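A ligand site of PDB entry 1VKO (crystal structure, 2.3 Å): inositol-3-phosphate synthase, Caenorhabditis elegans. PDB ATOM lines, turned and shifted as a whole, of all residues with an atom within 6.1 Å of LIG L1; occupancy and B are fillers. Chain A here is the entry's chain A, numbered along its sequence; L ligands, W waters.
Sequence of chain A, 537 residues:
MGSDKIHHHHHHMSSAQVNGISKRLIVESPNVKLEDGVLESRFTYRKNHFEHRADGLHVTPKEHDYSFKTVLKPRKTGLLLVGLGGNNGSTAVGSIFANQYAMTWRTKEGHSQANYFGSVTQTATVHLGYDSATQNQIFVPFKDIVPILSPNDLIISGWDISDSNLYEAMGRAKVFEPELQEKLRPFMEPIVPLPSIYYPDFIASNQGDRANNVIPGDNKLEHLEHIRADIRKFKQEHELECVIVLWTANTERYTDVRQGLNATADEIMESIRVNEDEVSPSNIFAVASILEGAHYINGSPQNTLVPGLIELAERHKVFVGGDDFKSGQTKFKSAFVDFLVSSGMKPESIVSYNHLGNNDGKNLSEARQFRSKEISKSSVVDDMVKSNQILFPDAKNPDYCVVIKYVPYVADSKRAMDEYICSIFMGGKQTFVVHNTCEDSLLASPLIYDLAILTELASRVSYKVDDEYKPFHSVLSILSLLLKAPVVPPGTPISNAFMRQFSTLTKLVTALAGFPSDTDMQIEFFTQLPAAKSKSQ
An oxygen (O1) of LIG L1 is in hydrogen-bond range of the backbone NH (N) of Gly 328.
NZ of Lys 377 is in salt-bridge range of O7 of LIG L1, at 2.6 Å.
The side-chain amino group (NZ) of Lys 484 lies within salt-bridge range of an oxygen (O6) of LIG L1 (2.6 Å).
NZ of Lys 414 is in salt-bridge range of O2 of LIG L1 (2.7 Å).
An oxygen (O2) of LIG L1 is in hydrogen-bond range of the backbone NH (N) of Gln 329.
The backbone NH (N) of Thr 330 is in hydrogen-bond range of an oxygen (O3) of LIG L1 (3.1 Å).
O3 of LIG L1 is in hydrogen-bond range of OG1 of Thr 330.
The backbone NH (N) of Ser 327 lies within hydrogen-bond range of an oxygen (O1) of LIG L1 (3.1 Å).
O4 of LIG L1 sits at hydrogen-bond distance from OG of Ser 327 (3.4 Å).
NZ of Lys 373 is in salt-bridge range of O6 of LIG L1 (3.1 Å).
The side-chain hydroxyl (OG) of Ser 327 lies within hydrogen-bond range of a nitrogen (N7) of LG2 L2, at 2.8 Å.
NZ of Lys 373 sits at hydrogen-bond distance from O13 of LG2 L2 (2.8 Å).
The backbone carbonyl oxygen (O) of Asp 440 is in hydrogen-bond range of a nitrogen (N7) of LG2 L2 (3.4 Å).
The side-chain carboxylate (OD1) of Asp 360 sits at hydrogen-bond distance from an oxygen (O13) of LG2 L2.
The side-chain amide oxygen (OE1) of Gln 329 lies within hydrogen-bond range of the side-chain amino group (NZ) of Lys 377, at 3.1 Å.
The side-chain amide oxygen (OD1) of Asn 354 sits at hydrogen-bond distance from the side-chain amino group (NZ) of Lys 377 (3.4 Å).
The backbone carbonyl oxygen of Phe 325 sits at hydrogen-bond distance from the side-chain amino group of Lys 484, 2.5 Å away.
The side-chain amino group (NZ) of Lys 484 lies within salt-bridge range of the side-chain carboxylate (OD2) of Asp 324.
OD1 of Asn 354 lies within hydrogen-bond range of NZ of Lys 414 (3.1 Å).
The backbone NH of Lys 414 is in hydrogen-bond range of the backbone carbonyl oxygen of Cys 438 (2.9 Å).
The side-chain amide oxygen (OE1) of Gln 329 is in hydrogen-bond range of the side-chain amide nitrogen (ND2) of Asn 354 (2.8 Å).
The side-chain amino group (NZ) of Lys 373 lies within salt-bridge range of the side-chain carboxylate (OD1) of Asp 324, at 2.6 Å.
Lys 326 touches LIG L1 (C to O1, 3.9 Å).
Lys 331 touches LIG L1 (N to O1, 3.98 Å).
Of the 20 residues printed, 10 come within 4 Å of LIG L1.
Water W1 lies within hydrogen-bond range of OG of Ser 327 (2.7 Å), OD1 of Asp 440 (2.8 Å), O2 of LIG L1 (3.0 Å) and N of Gly 328 (3.2 Å).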
ATOM      1  N   ASP A 324      18.181  -5.605  36.071  1.00  0.00           N
ATOM      2  CA  ASP A 324      17.426  -4.973  34.977  1.00  0.00           C
ATOM      3  C   ASP A 324      18.050  -5.264  33.605  1.00  0.00           C
ATOM      4  O   ASP A 324      19.174  -4.804  33.308  1.00  0.00           O
ATOM      5  CB  ASP A 324      17.295  -3.463  35.231  1.00  0.00           C
ATOM      6  CG  ASP A 324      16.151  -2.805  34.458  1.00  0.00           C
ATOM      7  OD1 ASP A 324      15.200  -3.505  34.012  1.00  0.00           O
ATOM      8  OD2 ASP A 324      16.093  -1.572  34.291  1.00  0.00           O
ATOM      9  N   PHE A 325      17.298  -6.017  32.780  1.00  0.00           N
ATOM     10  CA  PHE A 325      17.761  -6.404  31.457  1.00  0.00           C
ATOM     11  C   PHE A 325      18.288  -5.236  30.742  1.00  0.00           C
ATOM     12  O   PHE A 325      17.687  -4.139  30.738  1.00  0.00           O
ATOM     13  CB  PHE A 325      16.647  -7.004  30.588  1.00  0.00           C
ATOM     14  CG  PHE A 325      15.935  -8.203  31.182  1.00  0.00           C
ATOM     15  CD1 PHE A 325      16.645  -9.310  31.630  1.00  0.00           C
ATOM     16  CD2 PHE A 325      14.554  -8.227  31.261  1.00  0.00           C
ATOM     17  CE1 PHE A 325      15.960 -10.433  32.171  1.00  0.00           C
ATOM     18  CE2 PHE A 325      13.877  -9.356  31.807  1.00  0.00           C
ATOM     19  CZ  PHE A 325      14.597 -10.419  32.243  1.00  0.00           C
ATOM     20  N   LYS A 326      19.420  -5.455  30.110  1.00  0.00           N
ATOM     21  CA  LYS A 326      19.989  -4.459  29.258  1.00  0.00           C
ATOM     22  C   LYS A 326      19.760  -4.869  27.822  1.00  0.00           C
ATOM     23  O   LYS A 326      20.612  -5.532  27.194  1.00  0.00           O
ATOM     24  CB  LYS A 326      21.456  -4.313  29.565  1.00  0.00           C
ATOM     25  CG  LYS A 326      22.073  -3.212  28.842  1.00  0.00           C
ATOM     26  CD  LYS A 326      23.500  -3.593  28.577  1.00  0.00           C
ATOM     27  CE  LYS A 326      24.393  -3.207  29.703  1.00  0.00           C
ATOM     28  NZ  LYS A 326      25.809  -3.407  29.324  1.00  0.00           N
ATOM     29  N   SER A 327      18.597  -4.493  27.314  1.00  0.00           N
ATOM     30  CA  SER A 327      18.114  -5.070  26.060  1.00  0.00           C
ATOM     31  C   SER A 327      18.315  -4.170  24.805  1.00  0.00           C
ATOM     32  O   SER A 327      18.676  -4.689  23.727  1.00  0.00           O
ATOM     33  CB  SER A 327      16.635  -5.475  26.216  1.00  0.00           C
ATOM     34  OG  SER A 327      15.814  -4.389  26.622  1.00  0.00           O
ATOM     35  N   GLY A 328      18.091  -2.856  24.941  1.00  0.00           N
ATOM     36  CA  GLY A 328      17.948  -2.003  23.772  1.00  0.00           C
ATOM     37  C   GLY A 328      18.720  -0.694  23.807  1.00  0.00           C
ATOM     38  O   GLY A 328      19.905  -0.657  23.454  1.00  0.00           O
ATOM     39  N   GLN A 329      18.048   0.368  24.225  1.00  0.00           N
ATOM     40  CA  GLN A 329      18.616   1.720  24.199  1.00  0.00           C
ATOM     41  C   GLN A 329      19.867   1.882  25.101  1.00  0.00           C
ATOM     42  O   GLN A 329      20.812   2.595  24.752  1.00  0.00           O
ATOM     43  CB  GLN A 329      17.508   2.731  24.565  1.00  0.00           C
ATOM     44  CG  GLN A 329      17.976   4.159  24.760  1.00  0.00           C
ATOM     45  CD  GLN A 329      16.881   5.001  25.381  1.00  0.00           C
ATOM     46  OE1 GLN A 329      16.599   4.851  26.592  1.00  0.00           O
ATOM     47  NE2 GLN A 329      16.264   5.891  24.582  1.00  0.00           N
ATOM     48  N   THR A 330      19.852   1.194  26.237  1.00  0.00           N
ATOM     49  CA  THR A 330      20.958   1.185  27.205  1.00  0.00           C
ATOM     50  C   THR A 330      22.139   0.279  26.793  1.00  0.00           C
ATOM     51  O   THR A 330      23.282   0.589  27.127  1.00  0.00           O
ATOM     52  CB  THR A 330      20.417   0.807  28.625  1.00  0.00           C
ATOM     53  OG1 THR A 330      19.450   1.792  29.044  1.00  0.00           O
ATOM     54  CG2 THR A 330      21.530   0.897  29.694  1.00  0.00           C
ATOM     55  N   LYS A 331      21.848  -0.831  26.079  1.00  0.00           N
ATOM     56  CA  LYS A 331      22.894  -1.725  25.531  1.00  0.00           C
ATOM     57  C   LYS A 331      23.737  -0.891  24.542  1.00  0.00           C
ATOM     58  O   LYS A 331      24.977  -0.843  24.640  1.00  0.00           O
ATOM     59  CB  LYS A 331      22.269  -2.959  24.827  1.00  0.00           C
ATOM     60  CG  LYS A 331      23.200  -4.171  24.473  1.00  0.00           C
ATOM     61  CD  LYS A 331      22.429  -5.150  23.578  1.00  0.00           C
ATOM     62  CE  LYS A 331      23.130  -6.509  23.337  1.00  0.00           C
ATOM     63  NZ  LYS A 331      22.983  -7.519  24.464  1.00  0.00           N
ATOM     64  N   ASN A 354      11.802   7.321  25.276  1.00  0.00           N
ATOM     65  CA  ASN A 354      11.305   5.953  25.040  1.00  0.00           C
ATOM     66  C   ASN A 354       9.795   5.968  25.090  1.00  0.00           C
ATOM     67  O   ASN A 354       9.218   6.630  25.981  1.00  0.00           O
ATOM     68  CB  ASN A 354      11.818   4.969  26.089  1.00  0.00           C
ATOM     69  CG  ASN A 354      13.338   4.905  26.158  1.00  0.00           C
ATOM     70  OD1 ASN A 354      13.949   4.078  25.488  1.00  0.00           O
ATOM     71  ND2 ASN A 354      13.938   5.778  26.979  1.00  0.00           N
ATOM     72  N   LEU A 356       6.412   2.973  24.490  1.00  0.00           N
ATOM     73  CA  LEU A 356       5.930   1.586  24.251  1.00  0.00           C
ATOM     74  C   LEU A 356       4.496   1.419  24.751  1.00  0.00           C
ATOM     75  O   LEU A 356       3.976   2.243  25.527  1.00  0.00           O
ATOM     76  CB  LEU A 356       6.886   0.558  24.874  1.00  0.00           C
ATOM     77  CG  LEU A 356       7.022   0.393  26.390  1.00  0.00           C
ATOM     78  CD1 LEU A 356       8.066  -0.660  26.681  1.00  0.00           C
ATOM     79  CD2 LEU A 356       7.381   1.697  27.112  1.00  0.00           C
ATOM     80  N   ASP A 360       4.423  -3.691  30.186  1.00  0.00           N
ATOM     81  CA  ASP A 360       5.614  -3.098  30.793  1.00  0.00           C
ATOM     82  C   ASP A 360       5.446  -1.557  30.851  1.00  0.00           C
ATOM     83  O   ASP A 360       5.599  -0.956  31.925  1.00  0.00           O
ATOM     84  CB  ASP A 360       6.907  -3.557  30.061  1.00  0.00           C
ATOM     85  CG  ASP A 360       8.215  -3.016  30.681  1.00  0.00           C
ATOM     86  OD1 ASP A 360       8.229  -2.699  31.913  1.00  0.00           O
ATOM     87  OD2 ASP A 360       9.270  -2.846  30.014  1.00  0.00           O
ATOM     88  N   LYS A 373      13.187   2.253  37.193  1.00  0.00           N
ATOM     89  CA  LYS A 373      13.780   2.207  35.834  1.00  0.00           C
ATOM     90  C   LYS A 373      14.665   3.409  35.426  1.00  0.00           C
ATOM     91  O   LYS A 373      15.763   3.209  34.886  1.00  0.00           O
ATOM     92  CB  LYS A 373      12.674   1.986  34.804  1.00  0.00           C
ATOM     93  CG  LYS A 373      13.193   1.767  33.399  1.00  0.00           C
ATOM     94  CD  LYS A 373      13.709   0.331  33.175  1.00  0.00           C
ATOM     95  CE  LYS A 373      12.572  -0.695  33.178  1.00  0.00           C
ATOM     96  NZ  LYS A 373      13.192  -2.042  33.186  1.00  0.00           N
ATOM     97  N   LYS A 377      18.611   3.109  34.047  1.00  0.00           N
ATOM     98  CA  LYS A 377      18.925   3.664  32.716  1.00  0.00           C
ATOM     99  C   LYS A 377      19.962   4.829  32.763  1.00  0.00           C
ATOM    100  O   LYS A 377      20.859   4.928  31.893  1.00  0.00           O
ATOM    101  CB  LYS A 377      17.624   4.079  31.990  1.00  0.00           C
ATOM    102  CG  LYS A 377      16.701   2.900  31.523  1.00  0.00           C
ATOM    103  CD  LYS A 377      15.401   3.419  30.885  1.00  0.00           C
ATOM    104  CE  LYS A 377      15.585   3.840  29.414  1.00  0.00           C
ATOM    105  NZ  LYS A 377      15.146   2.786  28.420  1.00  0.00           N
ATOM    106  N   ILE A 404      10.468   7.724  29.816  1.00  0.00           N
ATOM    107  CA  ILE A 404       9.638   6.585  29.330  1.00  0.00           C
ATOM    108  C   ILE A 404       8.184   6.952  29.344  1.00  0.00           C
ATOM    109  O   ILE A 404       7.629   7.410  30.377  1.00  0.00           O
ATOM    110  CB  ILE A 404       9.831   5.294  30.133  1.00  0.00           C
ATOM    111  CG1 ILE A 404      11.316   4.891  30.214  1.00  0.00           C
ATOM    112  CG2 ILE A 404       8.953   4.168  29.526  1.00  0.00           C
ATOM    113  CD1 ILE A 404      11.612   3.920  31.365  1.00  0.00           C
ATOM    114  N   LYS A 414       8.870  -1.051  21.250  1.00  0.00           N
ATOM    115  CA  LYS A 414       9.317   0.236  21.881  1.00  0.00           C
ATOM    116  C   LYS A 414      10.134   1.083  20.912  1.00  0.00           C
ATOM    117  O   LYS A 414      10.783   0.559  19.994  1.00  0.00           O
ATOM    118  CB  LYS A 414       9.988   0.062  23.281  1.00  0.00           C
ATOM    119  CG  LYS A 414      11.492   0.058  23.336  1.00  0.00           C
ATOM    120  CD  LYS A 414      12.096   1.428  23.652  1.00  0.00           C
ATOM    121  CE  LYS A 414      13.564   1.287  24.102  1.00  0.00           C
ATOM    122  NZ  LYS A 414      13.707   0.996  25.558  1.00  0.00           N
ATOM    123  N   ALA A 416      13.017   4.010  20.786  1.00  0.00           N
ATOM    124  CA  ALA A 416      14.045   4.706  21.540  1.00  0.00           C
ATOM    125  C   ALA A 416      14.523   5.879  20.694  1.00  0.00           C
ATOM    126  O   ALA A 416      15.009   5.690  19.600  1.00  0.00           O
ATOM    127  CB  ALA A 416      15.197   3.751  21.912  1.00  0.00           C
ATOM    128  N   CYS A 438      12.919  -1.147  18.950  1.00  0.00           N
ATOM    129  CA  CYS A 438      13.274  -2.231  19.909  1.00  0.00           C
ATOM    130  C   CYS A 438      12.082  -3.145  20.173  1.00  0.00           C
ATOM    131  O   CYS A 438      11.128  -2.801  20.890  1.00  0.00           O
ATOM    132  CB  CYS A 438      13.750  -1.675  21.251  1.00  0.00           C
ATOM    133  SG  CYS A 438      15.263  -0.733  21.102  1.00  0.00           S
ATOM    134  N   ASP A 440      10.905  -5.179  22.205  1.00  0.00           N
ATOM    135  CA  ASP A 440      11.434  -5.457  23.555  1.00  0.00           C
ATOM    136  C   ASP A 440      11.501  -6.944  23.919  1.00  0.00           C
ATOM    137  O   ASP A 440      12.527  -7.419  24.400  1.00  0.00           O
ATOM    138  CB  ASP A 440      10.607  -4.725  24.613  1.00  0.00           C
ATOM    139  CG  ASP A 440      10.993  -3.267  24.725  1.00  0.00           C
ATOM    140  OD1 ASP A 440      12.156  -2.883  24.378  1.00  0.00           O
ATOM    141  OD2 ASP A 440      10.178  -2.429  25.162  1.00  0.00           O
ATOM    142  N   LEU A 443      14.075  -8.688  22.214  1.00  0.00           N
ATOM    143  CA  LEU A 443      15.362  -8.324  22.758  1.00  0.00           C
ATOM    144  C   LEU A 443      15.594  -9.012  24.112  1.00  0.00           C
ATOM    145  O   LEU A 443      16.675  -9.564  24.330  1.00  0.00           O
ATOM    146  CB  LEU A 443      15.515  -6.785  22.836  1.00  0.00           C
ATOM    147  CG  LEU A 443      15.924  -6.080  21.530  1.00  0.00           C
ATOM    148  CD1 LEU A 443      15.770  -4.558  21.585  1.00  0.00           C
ATOM    149  CD2 LEU A 443      17.351  -6.433  21.097  1.00  0.00           C
ATOM    150  N   LYS A 484      21.555  -3.730  33.240  1.00  0.00           N
ATOM    151  CA  LYS A 484      21.670  -2.286  33.158  1.00  0.00           C
ATOM    152  C   LYS A 484      22.336  -1.705  34.349  1.00  0.00           C
ATOM    153  O   LYS A 484      23.136  -0.757  34.218  1.00  0.00           O
ATOM    154  CB  LYS A 484      20.306  -1.635  33.135  1.00  0.00           C
ATOM    155  CG  LYS A 484      19.743  -1.429  31.778  1.00  0.00           C
ATOM    156  CD  LYS A 484      18.641  -0.375  31.857  1.00  0.00           C
ATOM    157  CE  LYS A 484      17.683  -0.599  30.717  1.00  0.00           C
ATOM    158  NZ  LYS A 484      16.831  -1.826  30.923  1.00  0.00           N
HETATM  159  P1  LIG L   1      16.759  -0.664  27.214  1.00  0.00           P
HETATM  160  O1  LIG L   1      18.014  -1.474  26.945  1.00  0.00           O
HETATM  161  O2  LIG L   1      15.967  -0.494  25.938  1.00  0.00           O
HETATM  162  O3  LIG L   1      17.145   0.715  27.731  1.00  0.00           O
HETATM  163  O4  LIG L   1      15.816  -1.471  28.277  1.00  0.00           O
HETATM  164  P2  LIG L   1      14.356  -1.001  28.857  1.00  0.00           P
HETATM  165  O5  LIG L   1      13.287  -1.751  28.080  1.00  0.00           O
HETATM  166  O6  LIG L   1      14.311  -1.309  30.344  1.00  0.00           O
HETATM  167  O7  LIG L   1      14.025   0.489  28.696  1.00  0.00           O
HETATM  168  P1  LG2 L   2       4.657  -7.813  31.197  1.00  0.00           P
HETATM  169  O1  LG2 L   2       3.609  -7.023  31.812  1.00  0.00           O
HETATM  170  O2  LG2 L   2       4.189  -8.282  29.883  1.00  0.00           O
HETATM  171  O3  LG2 L   2       5.015  -8.990  32.201  1.00  0.00           O
HETATM  172  C1  LG2 L   2       4.736  -8.856  33.567  1.00  0.00           C
HETATM  173  C2  LG2 L   2       3.984 -10.098  33.995  1.00  0.00           C
HETATM  174  O4  LG2 L   2       4.255 -10.336  35.358  1.00  0.00           O
HETATM  175  C3  LG2 L   2       2.502  -9.942  33.877  1.00  0.00           C
HETATM  176  O5  LG2 L   2       2.033 -11.231  33.490  1.00  0.00           O
HETATM  177  C4  LG2 L   2       1.987  -9.724  35.273  1.00  0.00           C
HETATM  178  O6  LG2 L   2       0.821 -10.542  35.361  1.00  0.00           O
HETATM  179  C5  LG2 L   2       3.078 -10.371  36.110  1.00  0.00           C
HETATM  180  N1  LG2 L   2       3.281  -9.940  37.521  1.00  0.00           N
HETATM  181  C6  LG2 L   2       3.189  -8.708  38.087  1.00  0.00           C
HETATM  182  N2  LG2 L   2       3.448  -8.824  39.409  1.00  0.00           N
HETATM  183  C7  LG2 L   2       3.697 -10.108  39.731  1.00  0.00           C
HETATM  184  C8  LG2 L   2       3.975 -10.789  40.929  1.00  0.00           C
HETATM  185  N3  LG2 L   2       3.997 -10.186  42.131  1.00  0.00           N
HETATM  186  N4  LG2 L   2       4.152 -12.149  40.898  1.00  0.00           N
HETATM  187  C9  LG2 L   2       4.032 -12.837  39.717  1.00  0.00           C
HETATM  188  N5  LG2 L   2       3.715 -12.165  38.580  1.00  0.00           N
HETATM  189  C10 LG2 L   2       3.565 -10.825  38.558  1.00  0.00           C
HETATM  190  O7  LG2 L   2       6.049  -7.001  31.077  1.00  0.00           O
HETATM  191  P2  LG2 L   2       7.285  -7.631  30.296  1.00  0.00           P
HETATM  192  O8  LG2 L   2       7.112  -9.102  30.322  1.00  0.00           O
HETATM  193  O9  LG2 L   2       7.369  -6.948  28.993  1.00  0.00           O
HETATM  194  O10 LG2 L   2       8.587  -7.362  31.219  1.00  0.00           O
HETATM  195  C11 LG2 L   2       8.561  -7.656  32.613  1.00  0.00           C
HETATM  196  C12 LG2 L   2       9.619  -6.893  33.427  1.00  0.00           C
HETATM  197  O11 LG2 L   2      10.875  -6.965  32.811  1.00  0.00           O
HETATM  198  C13 LG2 L   2       9.316  -5.407  33.619  1.00  0.00           C
HETATM  199  O12 LG2 L   2       9.646  -5.040  34.929  1.00  0.00           O
HETATM  200  C14 LG2 L   2      10.348  -4.724  32.753  1.00  0.00           C
HETATM  201  O13 LG2 L   2      10.781  -3.449  33.214  1.00  0.00           O
HETATM  202  C15 LG2 L   2      11.489  -5.701  32.858  1.00  0.00           C
HETATM  203  N6  LG2 L   2      12.376  -5.378  31.750  1.00  0.00           N
HETATM  204  C16 LG2 L   2      11.945  -5.494  30.466  1.00  0.00           C
HETATM  205  C17 LG2 L   2      12.794  -5.147  29.437  1.00  0.00           C
HETATM  206  C18 LG2 L   2      12.419  -5.658  28.091  1.00  0.00           C
HETATM  207  O14 LG2 L   2      11.171  -6.328  28.028  1.00  0.00           O
HETATM  208  N7  LG2 L   2      13.245  -5.476  27.060  1.00  0.00           N
HETATM  209  C19 LG2 L   2      14.101  -4.701  29.695  1.00  0.00           C
HETATM  210  C20 LG2 L   2      14.511  -4.563  31.000  1.00  0.00           C
HETATM  211  C21 LG2 L   2      13.633  -4.905  32.038  1.00  0.00           C
HETATM  212  O   HOH W   1      14.934  -2.914  24.565  1.00  0.00           O
